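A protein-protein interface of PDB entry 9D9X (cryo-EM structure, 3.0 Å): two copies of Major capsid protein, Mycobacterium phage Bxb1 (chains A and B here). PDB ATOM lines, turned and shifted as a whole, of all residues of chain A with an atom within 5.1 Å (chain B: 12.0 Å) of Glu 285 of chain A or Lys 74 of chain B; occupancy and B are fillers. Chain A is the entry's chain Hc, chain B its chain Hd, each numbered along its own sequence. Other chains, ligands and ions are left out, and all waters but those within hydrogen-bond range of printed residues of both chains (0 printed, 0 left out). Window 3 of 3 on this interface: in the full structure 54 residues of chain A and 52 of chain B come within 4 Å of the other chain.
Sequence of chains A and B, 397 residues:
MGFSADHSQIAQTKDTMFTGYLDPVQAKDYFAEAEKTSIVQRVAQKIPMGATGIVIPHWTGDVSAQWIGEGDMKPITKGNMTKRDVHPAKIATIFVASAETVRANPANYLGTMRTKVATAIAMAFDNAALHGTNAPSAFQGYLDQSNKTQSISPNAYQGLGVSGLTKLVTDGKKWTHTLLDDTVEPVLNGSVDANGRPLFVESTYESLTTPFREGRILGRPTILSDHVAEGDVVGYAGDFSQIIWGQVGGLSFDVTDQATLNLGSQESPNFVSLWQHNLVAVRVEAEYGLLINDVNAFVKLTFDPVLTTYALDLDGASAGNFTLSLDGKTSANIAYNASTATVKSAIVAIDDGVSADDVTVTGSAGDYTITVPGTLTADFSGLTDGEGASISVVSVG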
ATOM      1  N   LYS A  90      31.678 -16.769  23.194  1.00  0.00           N
ATOM      2  CA  LYS A  90      30.416 -16.304  22.620  1.00  0.00           C
ATOM      3  C   LYS A  90      30.621 -15.010  21.838  1.00  0.00           C
ATOM      4  O   LYS A  90      31.207 -14.061  22.356  1.00  0.00           O
ATOM      5  CB  LYS A  90      29.460 -16.099  23.805  1.00  0.00           C
ATOM      6  CG  LYS A  90      28.050 -15.623  23.451  1.00  0.00           C
ATOM      7  CD  LYS A  90      27.192 -16.681  22.755  1.00  0.00           C
ATOM      8  CE  LYS A  90      26.867 -17.849  23.693  1.00  0.00           C
ATOM      9  NZ  LYS A  90      25.829 -18.739  23.117  1.00  0.00           N
ATOM     10  N   ILE A  91      30.094 -14.942  20.621  1.00  0.00           N
ATOM     11  CA  ILE A  91      29.983 -13.706  19.841  1.00  0.00           C
ATOM     12  C   ILE A  91      28.517 -13.387  19.609  1.00  0.00           C
ATOM     13  O   ILE A  91      27.723 -14.281  19.319  1.00  0.00           O
ATOM     14  CB  ILE A  91      30.798 -13.774  18.542  1.00  0.00           C
ATOM     15  CG1 ILE A  91      30.646 -12.466  17.756  1.00  0.00           C
ATOM     16  CG2 ILE A  91      30.432 -14.974  17.660  1.00  0.00           C
ATOM     17  CD1 ILE A  91      31.756 -12.227  16.738  1.00  0.00           C
ATOM     18  N   ALA A  92      28.133 -12.125  19.774  1.00  0.00           N
ATOM     19  CA  ALA A  92      26.737 -11.727  19.692  1.00  0.00           C
ATOM     20  C   ALA A  92      26.546 -10.252  19.345  1.00  0.00           C
ATOM     21  O   ALA A  92      27.423  -9.427  19.588  1.00  0.00           O
ATOM     22  CB  ALA A  92      26.097 -12.057  21.037  1.00  0.00           C
ATOM     23  N   THR A  93      25.387  -9.901  18.796  1.00  0.00           N
ATOM     24  CA  THR A  93      25.028  -8.515  18.460  1.00  0.00           C
ATOM     25  C   THR A  93      23.513  -8.331  18.390  1.00  0.00           C
ATOM     26  O   THR A  93      22.782  -9.307  18.212  1.00  0.00           O
ATOM     27  CB  THR A  93      25.720  -8.108  17.156  1.00  0.00           C
ATOM     28  OG1 THR A  93      25.725  -6.716  17.012  1.00  0.00           O
ATOM     29  CG2 THR A  93      25.092  -8.693  15.896  1.00  0.00           C
ATOM     30  N   ILE A  94      23.027  -7.100  18.535  1.00  0.00           N
ATOM     31  CA  ILE A  94      21.600  -6.747  18.507  1.00  0.00           C
ATOM     32  C   ILE A  94      21.365  -5.602  17.525  1.00  0.00           C
ATOM     33  O   ILE A  94      22.139  -4.652  17.496  1.00  0.00           O
ATOM     34  CB  ILE A  94      21.116  -6.390  19.930  1.00  0.00           C
ATOM     35  CG1 ILE A  94      21.095  -7.655  20.810  1.00  0.00           C
ATOM     36  CG2 ILE A  94      19.729  -5.726  19.944  1.00  0.00           C
ATOM     37  CD1 ILE A  94      20.796  -7.408  22.286  1.00  0.00           C
ATOM     38  N   GLY A 250      25.534 -23.438  15.720  1.00  0.00           N
ATOM     39  CA  GLY A 250      25.570 -22.490  14.606  1.00  0.00           C
ATOM     40  C   GLY A 250      24.875 -21.174  14.928  1.00  0.00           C
ATOM     41  O   GLY A 250      24.510 -20.928  16.078  1.00  0.00           O
ATOM     42  N   LEU A 251      24.684 -20.318  13.924  1.00  0.00           N
ATOM     43  CA  LEU A 251      23.996 -19.033  14.076  1.00  0.00           C
ATOM     44  C   LEU A 251      22.585 -19.229  14.610  1.00  0.00           C
ATOM     45  O   LEU A 251      21.838 -20.075  14.124  1.00  0.00           O
ATOM     46  CB  LEU A 251      23.918 -18.308  12.726  1.00  0.00           C
ATOM     47  CG  LEU A 251      25.238 -17.658  12.312  1.00  0.00           C
ATOM     48  CD1 LEU A 251      25.236 -17.387  10.812  1.00  0.00           C
ATOM     49  CD2 LEU A 251      25.436 -16.328  13.028  1.00  0.00           C
ATOM     50  N   SER A 252      22.204 -18.413  15.586  1.00  0.00           N
ATOM     51  CA  SER A 252      20.886 -18.450  16.213  1.00  0.00           C
ATOM     52  C   SER A 252      20.330 -17.041  16.371  1.00  0.00           C
ATOM     53  O   SER A 252      21.061 -16.124  16.736  1.00  0.00           O
ATOM     54  CB  SER A 252      20.982 -19.184  17.545  1.00  0.00           C
ATOM     55  OG  SER A 252      21.888 -18.537  18.415  1.00  0.00           O
ATOM     56  N   ARG A 283      18.178 -10.173  18.054  1.00  0.00           N
ATOM     57  CA  ARG A 283      19.306 -10.625  18.877  1.00  0.00           C
ATOM     58  C   ARG A 283      19.931 -11.849  18.233  1.00  0.00           C
ATOM     59  O   ARG A 283      19.210 -12.748  17.819  1.00  0.00           O
ATOM     60  CB  ARG A 283      18.742 -10.888  20.281  1.00  0.00           C
ATOM     61  CG  ARG A 283      19.578 -11.713  21.272  1.00  0.00           C
ATOM     62  CD  ARG A 283      19.042 -11.600  22.716  1.00  0.00           C
ATOM     63  NE  ARG A 283      17.570 -11.803  22.848  1.00  0.00           N
ATOM     64  CZ  ARG A 283      16.602 -10.938  23.142  1.00  0.00           C
ATOM     65  NH1 ARG A 283      15.393 -11.381  23.248  1.00  0.00           N
ATOM     66  NH2 ARG A 283      16.778  -9.662  23.332  1.00  0.00           N
ATOM     67  N   VAL A 284      21.255 -11.865  18.106  1.00  0.00           N
ATOM     68  CA  VAL A 284      21.994 -12.852  17.300  1.00  0.00           C
ATOM     69  C   VAL A 284      23.177 -13.422  18.077  1.00  0.00           C
ATOM     70  O   VAL A 284      23.930 -12.652  18.666  1.00  0.00           O
ATOM     71  CB  VAL A 284      22.506 -12.207  16.005  1.00  0.00           C
ATOM     72  CG1 VAL A 284      22.987 -13.278  15.033  1.00  0.00           C
ATOM     73  CG2 VAL A 284      21.436 -11.366  15.307  1.00  0.00           C
ATOM     74  N   GLU A 285      23.382 -14.741  18.063  1.00  0.00           N
ATOM     75  CA  GLU A 285      24.503 -15.411  18.741  1.00  0.00           C
ATOM     76  C   GLU A 285      25.132 -16.545  17.923  1.00  0.00           C
ATOM     77  O   GLU A 285      24.425 -17.332  17.288  1.00  0.00           O
ATOM     78  CB  GLU A 285      24.070 -16.049  20.069  1.00  0.00           C
ATOM     79  CG  GLU A 285      23.506 -15.105  21.140  1.00  0.00           C
ATOM     80  CD  GLU A 285      23.354 -15.782  22.523  1.00  0.00           C
ATOM     81  OE1 GLU A 285      23.676 -16.985  22.677  1.00  0.00           O
ATOM     82  OE2 GLU A 285      22.935 -15.090  23.482  1.00  0.00           O
ATOM     83  N   ALA A 286      26.452 -16.706  18.056  1.00  0.00           N
ATOM     84  CA  ALA A 286      27.219 -17.889  17.671  1.00  0.00           C
ATOM     85  C   ALA A 286      28.383 -18.127  18.651  1.00  0.00           C
ATOM     86  O   ALA A 286      28.712 -17.256  19.457  1.00  0.00           O
ATOM     87  CB  ALA A 286      27.702 -17.731  16.231  1.00  0.00           C
ATOM     88  N   GLU A 287      28.995 -19.310  18.630  1.00  0.00           N
ATOM     89  CA  GLU A 287      30.002 -19.713  19.620  1.00  0.00           C
ATOM     90  C   GLU A 287      31.185 -20.474  19.002  1.00  0.00           C
ATOM     91  O   GLU A 287      30.990 -21.441  18.270  1.00  0.00           O
ATOM     92  CB  GLU A 287      29.255 -20.514  20.688  1.00  0.00           C
ATOM     93  CG  GLU A 287      30.097 -21.008  21.864  1.00  0.00           C
ATOM     94  CD  GLU A 287      29.224 -21.563  23.005  1.00  0.00           C
ATOM     95  OE1 GLU A 287      28.075 -21.094  23.192  1.00  0.00           O
ATOM     96  OE2 GLU A 287      29.698 -22.449  23.750  1.00  0.00           O
ATOM     97  N   VAL B  63      28.233  -2.940   9.577  1.00  0.00           N
ATOM     98  CA  VAL B  63      27.643  -3.770  10.641  1.00  0.00           C
ATOM     99  C   VAL B  63      28.733  -4.404  11.511  1.00  0.00           C
ATOM    100  O   VAL B  63      29.807  -4.721  11.007  1.00  0.00           O
ATOM    101  CB  VAL B  63      26.737  -4.834  10.009  1.00  0.00           C
ATOM    102  CG1 VAL B  63      26.126  -5.790  11.030  1.00  0.00           C
ATOM    103  CG2 VAL B  63      25.579  -4.156   9.272  1.00  0.00           C
ATOM    104  N   SER B  64      28.497  -4.600  12.810  1.00  0.00           N
ATOM    105  CA  SER B  64      29.515  -5.081  13.763  1.00  0.00           C
ATOM    106  C   SER B  64      28.986  -6.078  14.797  1.00  0.00           C
ATOM    107  O   SER B  64      27.801  -6.100  15.130  1.00  0.00           O
ATOM    108  CB  SER B  64      30.129  -3.896  14.508  1.00  0.00           C
ATOM    109  OG  SER B  64      30.797  -3.029  13.612  1.00  0.00           O
ATOM    110  N   ALA B  65      29.889  -6.878  15.356  1.00  0.00           N
ATOM    111  CA  ALA B  65      29.641  -7.815  16.448  1.00  0.00           C
ATOM    112  C   ALA B  65      30.822  -7.813  17.421  1.00  0.00           C
ATOM    113  O   ALA B  65      31.894  -7.321  17.077  1.00  0.00           O
ATOM    114  CB  ALA B  65      29.383  -9.200  15.853  1.00  0.00           C
ATOM    115  N   GLN B  66      30.653  -8.344  18.630  1.00  0.00           N
ATOM    116  CA  GLN B  66      31.723  -8.388  19.625  1.00  0.00           C
ATOM    117  C   GLN B  66      31.741  -9.696  20.396  1.00  0.00           C
ATOM    118  O   GLN B  66      30.715 -10.348  20.575  1.00  0.00           O
ATOM    119  CB  GLN B  66      31.610  -7.232  20.618  1.00  0.00           C
ATOM    120  CG  GLN B  66      31.645  -5.859  19.942  1.00  0.00           C
ATOM    121  CD  GLN B  66      31.671  -4.715  20.939  1.00  0.00           C
ATOM    122  OE1 GLN B  66      31.927  -4.872  22.124  1.00  0.00           O
ATOM    123  NE2 GLN B  66      31.398  -3.507  20.503  1.00  0.00           N
ATOM    124  N   TRP B  67      32.921 -10.052  20.882  1.00  0.00           N
ATOM    125  CA  TRP B  67      33.118 -11.169  21.787  1.00  0.00           C
ATOM    126  C   TRP B  67      32.700 -10.790  23.201  1.00  0.00           C
ATOM    127  O   TRP B  67      33.063  -9.724  23.693  1.00  0.00           O
ATOM    128  CB  TRP B  67      34.587 -11.569  21.723  1.00  0.00           C
ATOM    129  CG  TRP B  67      34.996 -12.031  20.368  1.00  0.00           C
ATOM    130  CD1 TRP B  67      35.626 -11.297  19.428  1.00  0.00           C
ATOM    131  CD2 TRP B  67      34.720 -13.315  19.756  1.00  0.00           C
ATOM    132  NE1 TRP B  67      35.723 -12.033  18.266  1.00  0.00           N
ATOM    133  CE2 TRP B  67      35.122 -13.260  18.400  1.00  0.00           C
ATOM    134  CE3 TRP B  67      34.125 -14.508  20.205  1.00  0.00           C
ATOM    135  CZ2 TRP B  67      34.875 -14.302  17.509  1.00  0.00           C
ATOM    136  CZ3 TRP B  67      33.905 -15.583  19.327  1.00  0.00           C
ATOM    137  CH2 TRP B  67      34.261 -15.470  17.975  1.00  0.00           C
ATOM    138  N   ILE B  68      31.957 -11.664  23.872  1.00  0.00           N
ATOM    139  CA  ILE B  68      31.399 -11.422  25.203  1.00  0.00           C
ATOM    140  C   ILE B  68      31.587 -12.638  26.109  1.00  0.00           C
ATOM    141  O   ILE B  68      31.554 -13.779  25.656  1.00  0.00           O
ATOM    142  CB  ILE B  68      29.918 -11.018  25.103  1.00  0.00           C
ATOM    143  CG1 ILE B  68      29.083 -12.027  24.296  1.00  0.00           C
ATOM    144  CG2 ILE B  68      29.773  -9.600  24.541  1.00  0.00           C
ATOM    145  CD1 ILE B  68      27.583 -11.868  24.528  1.00  0.00           C
ATOM    146  N   GLY B  69      31.795 -12.413  27.403  1.00  0.00           N
ATOM    147  CA  GLY B  69      31.826 -13.481  28.400  1.00  0.00           C
ATOM    148  C   GLY B  69      30.431 -13.944  28.808  1.00  0.00           C
ATOM    149  O   GLY B  69      29.420 -13.365  28.418  1.00  0.00           O
ATOM    150  N   GLU B  70      30.347 -14.977  29.639  1.00  0.00           N
ATOM    151  CA  GLU B  70      29.082 -15.341  30.277  1.00  0.00           C
ATOM    152  C   GLU B  70      28.612 -14.189  31.180  1.00  0.00           C
ATOM    153  O   GLU B  70      29.374 -13.690  32.010  1.00  0.00           O
ATOM    154  CB  GLU B  70      29.244 -16.664  31.035  1.00  0.00           C
ATOM    155  CG  GLU B  70      27.968 -17.081  31.781  1.00  0.00           C
ATOM    156  CD  GLU B  70      28.065 -18.455  32.465  1.00  0.00           C
ATOM    157  OE1 GLU B  70      29.145 -19.080  32.492  1.00  0.00           O
ATOM    158  OE2 GLU B  70      27.044 -18.929  33.005  1.00  0.00           O
ATOM    159  N   GLY B  71      27.362 -13.756  31.010  1.00  0.00           N
ATOM    160  CA  GLY B  71      26.757 -12.670  31.781  1.00  0.00           C
ATOM    161  C   GLY B  71      27.184 -11.257  31.376  1.00  0.00           C
ATOM    162  O   GLY B  71      26.724 -10.293  31.979  1.00  0.00           O
ATOM    163  N   ASP B  72      28.043 -11.088  30.373  1.00  0.00           N
ATOM    164  CA  ASP B  72      28.253  -9.781  29.747  1.00  0.00           C
ATOM    165  C   ASP B  72      27.042  -9.401  28.899  1.00  0.00           C
ATOM    166  O   ASP B  72      26.362 -10.272  28.353  1.00  0.00           O
ATOM    167  CB  ASP B  72      29.522  -9.786  28.894  1.00  0.00           C
ATOM    168  CG  ASP B  72      30.814  -9.753  29.702  1.00  0.00           C
ATOM    169  OD1 ASP B  72      30.800  -9.251  30.849  1.00  0.00           O
ATOM    170  OD2 ASP B  72      31.861 -10.161  29.151  1.00  0.00           O
ATOM    171  N   MET B  73      26.768  -8.103  28.773  1.00  0.00           N
ATOM    172  CA  MET B  73      25.553  -7.627  28.114  1.00  0.00           C
ATOM    173  C   MET B  73      25.856  -7.209  26.672  1.00  0.00           C
ATOM    174  O   MET B  73      26.797  -6.458  26.427  1.00  0.00           O
ATOM    175  CB  MET B  73      24.869  -6.523  28.945  1.00  0.00           C
ATOM    176  CG  MET B  73      24.559  -6.853  30.435  1.00  0.00           C
ATOM    177  SD  MET B  73      23.758  -8.421  30.920  1.00  0.00           S
ATOM    178  CE  MET B  73      22.311  -8.503  29.848  1.00  0.00           C
ATOM    179  N   LYS B  74      25.087  -7.730  25.710  1.00  0.00           N
ATOM    180  CA  LYS B  74      25.336  -7.630  24.264  1.00  0.00           C
ATOM    181  C   LYS B  74      25.400  -6.177  23.747  1.00  0.00           C
ATOM    182  O   LYS B  74      24.680  -5.327  24.264  1.00  0.00           O
ATOM    183  CB  LYS B  74      24.224  -8.363  23.502  1.00  0.00           C
ATOM    184  CG  LYS B  74      24.332  -9.888  23.405  1.00  0.00           C
ATOM    185  CD  LYS B  74      23.926 -10.693  24.645  1.00  0.00           C
ATOM    186  CE  LYS B  74      23.784 -12.164  24.237  1.00  0.00           C
ATOM    187  NZ  LYS B  74      23.285 -13.041  25.325  1.00  0.00           N
ATOM    188  N   PRO B  75      26.188  -5.882  22.698  1.00  0.00           N
ATOM    189  CA  PRO B  75      26.241  -4.581  22.029  1.00  0.00           C
ATOM    190  C   PRO B  75      25.132  -4.390  20.979  1.00  0.00           C
ATOM    191  O   PRO B  75      24.506  -5.356  20.550  1.00  0.00           O
ATOM    192  CB  PRO B  75      27.603  -4.577  21.349  1.00  0.00           C
ATOM    193  CG  PRO B  75      27.724  -6.025  20.897  1.00  0.00           C
ATOM    194  CD  PRO B  75      27.123  -6.791  22.065  1.00  0.00           C
ATOM    195  N   ILE B  76      24.931  -3.153  20.509  1.00  0.00           N
ATOM    196  CA  ILE B  76      23.895  -2.778  19.524  1.00  0.00           C
ATOM    197  C   ILE B  76      24.510  -2.173  18.258  1.00  0.00           C
ATOM    198  O   ILE B  76      25.441  -1.376  18.348  1.00  0.00           O
ATOM    199  CB  ILE B  76      22.856  -1.841  20.171  1.00  0.00           C
ATOM    200  CG1 ILE B  76      22.047  -2.617  21.229  1.00  0.00           C
ATOM    201  CG2 ILE B  76      21.892  -1.241  19.137  1.00  0.00           C
ATOM    202  CD1 ILE B  76      21.226  -1.729  22.159  1.00  0.00           C
ATOM    203  N   THR B  77      23.991  -2.511  17.075  1.00  0.00           N
ATOM    204  CA  THR B  77      24.537  -2.112  15.764  1.00  0.00           C
ATOM    205  C   THR B  77      23.463  -1.679  14.756  1.00  0.00           C
ATOM    206  O   THR B  77      22.281  -1.953  14.950  1.00  0.00           O
ATOM    207  CB  THR B  77      25.409  -3.246  15.215  1.00  0.00           C
ATOM    208  OG1 THR B  77      26.230  -2.763  14.178  1.00  0.00           O
ATOM    209  CG2 THR B  77      24.612  -4.416  14.648  1.00  0.00           C
ATOM    210  N   LYS B  78      23.846  -0.977  13.681  1.00  0.00           N
ATOM    211  CA  LYS B  78      22.933  -0.411  12.672  1.00  0.00           C
ATOM    212  C   LYS B  78      23.510  -0.484  11.257  1.00  0.00           C
ATOM    213  O   LYS B  78      24.697  -0.228  11.072  1.00  0.00           O
ATOM    214  CB  LYS B  78      22.642   1.037  13.077  1.00  0.00           C
ATOM    215  CG  LYS B  78      21.457   1.651  12.332  1.00  0.00           C
ATOM    216  CD  LYS B  78      21.376   3.145  12.646  1.00  0.00           C
ATOM    217  CE  LYS B  78      20.233   3.773  11.858  1.00  0.00           C
ATOM    218  NZ  LYS B  78      20.166   5.232  12.091  1.00  0.00           N
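N of Ile 68 of chain B sits at hydrogen-bond distance from O of Lys 90 of chain A (2.9 Å). O of Gln 66 of chain B lies within hydrogen-bond range of N of Ala 92 of chain A (3.2 Å). The side-chain hydroxyl (OG1) of Thr 93 of chain A sits at hydrogen-bond distance from the backbone carbonyl oxygen (O) of Ser 64 of chain B (2.9 Å). N of Ile 94 of chain A sits at hydrogen-bond distance from O of Pro 75 of chain B, at 3.0 Å. N of Thr 77 of chain B sits at hydrogen-bond distance from O of Ile 94 of chain A (2.9 Å). The side-chain amino group (NZ) of Lys 74 of chain B is in salt-bridge range of the side-chain carboxylate (OE2) of Glu 285 of chain A (2.8 Å).
The side-chain carboxylate (OE1) of Glu 285 of chain A lies within salt-bridge range of the side-chain amino group (NZ) of Lys 90 of chain A. The side-chain amino group (NZ) of Lys 90 of chain A is in salt-bridge range of the side-chain carboxylate (OE1) of Glu 287 of chain A, 3.3 Å away. O of Ala 286 of chain A is in hydrogen-bond range of N of Ile 91 of chain A, at 2.9 Å. The backbone carbonyl oxygen (O) of Thr 93 of chain A is in hydrogen-bond range of the backbone NH (N) of Val 284 of chain A, 3.0 Å away. The backbone NH (N) of Ser 252 of chain A sits at hydrogen-bond distance from the backbone carbonyl oxygen (O) of Glu 285 of chain A (3.0 Å). N of Ser 64 of chain B lies within hydrogen-bond range of OG1 of Thr 77 of chain B, at 3.2 Å.
Lys 90 of chain A touches Trp 67 of chain B. Gln 66 of chain B touches Ile 91 of chain A (O to CA, 3.5 Å). Ile 91 of chain A touches Trp 67 of chain B (CB to CZ3, 3.7 Å). Ile 68 of chain B touches Ala 92 of chain A (CD1 to CB, 3.8 Å). Pro 75 of chain B touches Ala 92 of chain A (CD to O, 3.6 Å). Thr 93 of chain A touches Ala 65 of chain B. Pro 75 of chain B touches Thr 93 of chain A (O to C, 3.8 Å). CG2 of Thr 77 of chain B touches OG1 of Thr 93 of chain A, at 3.5 Å. Ile 94 of chain A touches Lys 74 of chain B. Ile 94 of chain A touches Ile 76 of chain B (O to CA, 3.3 Å).
Ala 92 of chain A touches just these residues of chain B: Gln 66, Ile 68, Lys 74 and Pro 75. Printed residues of chain B within 4 Å of Ile 94 of chain A: Lys 74, Pro 75, Ile 76 and Thr 77. No residue of chain B comes within 4 Å of Gly 250 of chain A. No residue of chain B comes within 4 Å of Leu 251 of chain A. Of the printed residues of chain B, Glu 285 of chain A touches Lys 74 (2.8 Å). No residue of chain B comes within 4 Å of Ala 286 of chain A. Of the printed residues of chain A, Trp 67 of chain B touches Lys 90 and Ile 91. Of the printed residues of chain A, Ile 68 of chain B touches Lys 90 (2.9 Å) and Ala 92 (3.8 Å). Of chain A, only Ala 92, Ile 94 and Glu 285 come within 4 Å of Lys 74 of chain B. The nearest printed residue of chain A that does not touch Trp 67 of chain B is Ala 92 of chain A (5.3 Å).
Hydrophobic or aromatic side chains of chain B that line the printed part of chain A: Ala 65, Trp 67, Ile 68, Pro 75 and Ile 76. Hydrophobic or aromatic side chains of chain A that line the printed part of chain B: Ile 91, Ala 92 and Ile 94. Among the printed residues, 18 pairs touch across the chains.
No position is printed for both chains. Of the 18 pairs that touch across the chains among the printed residues, none has its exchanged pair printed and touching as well.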
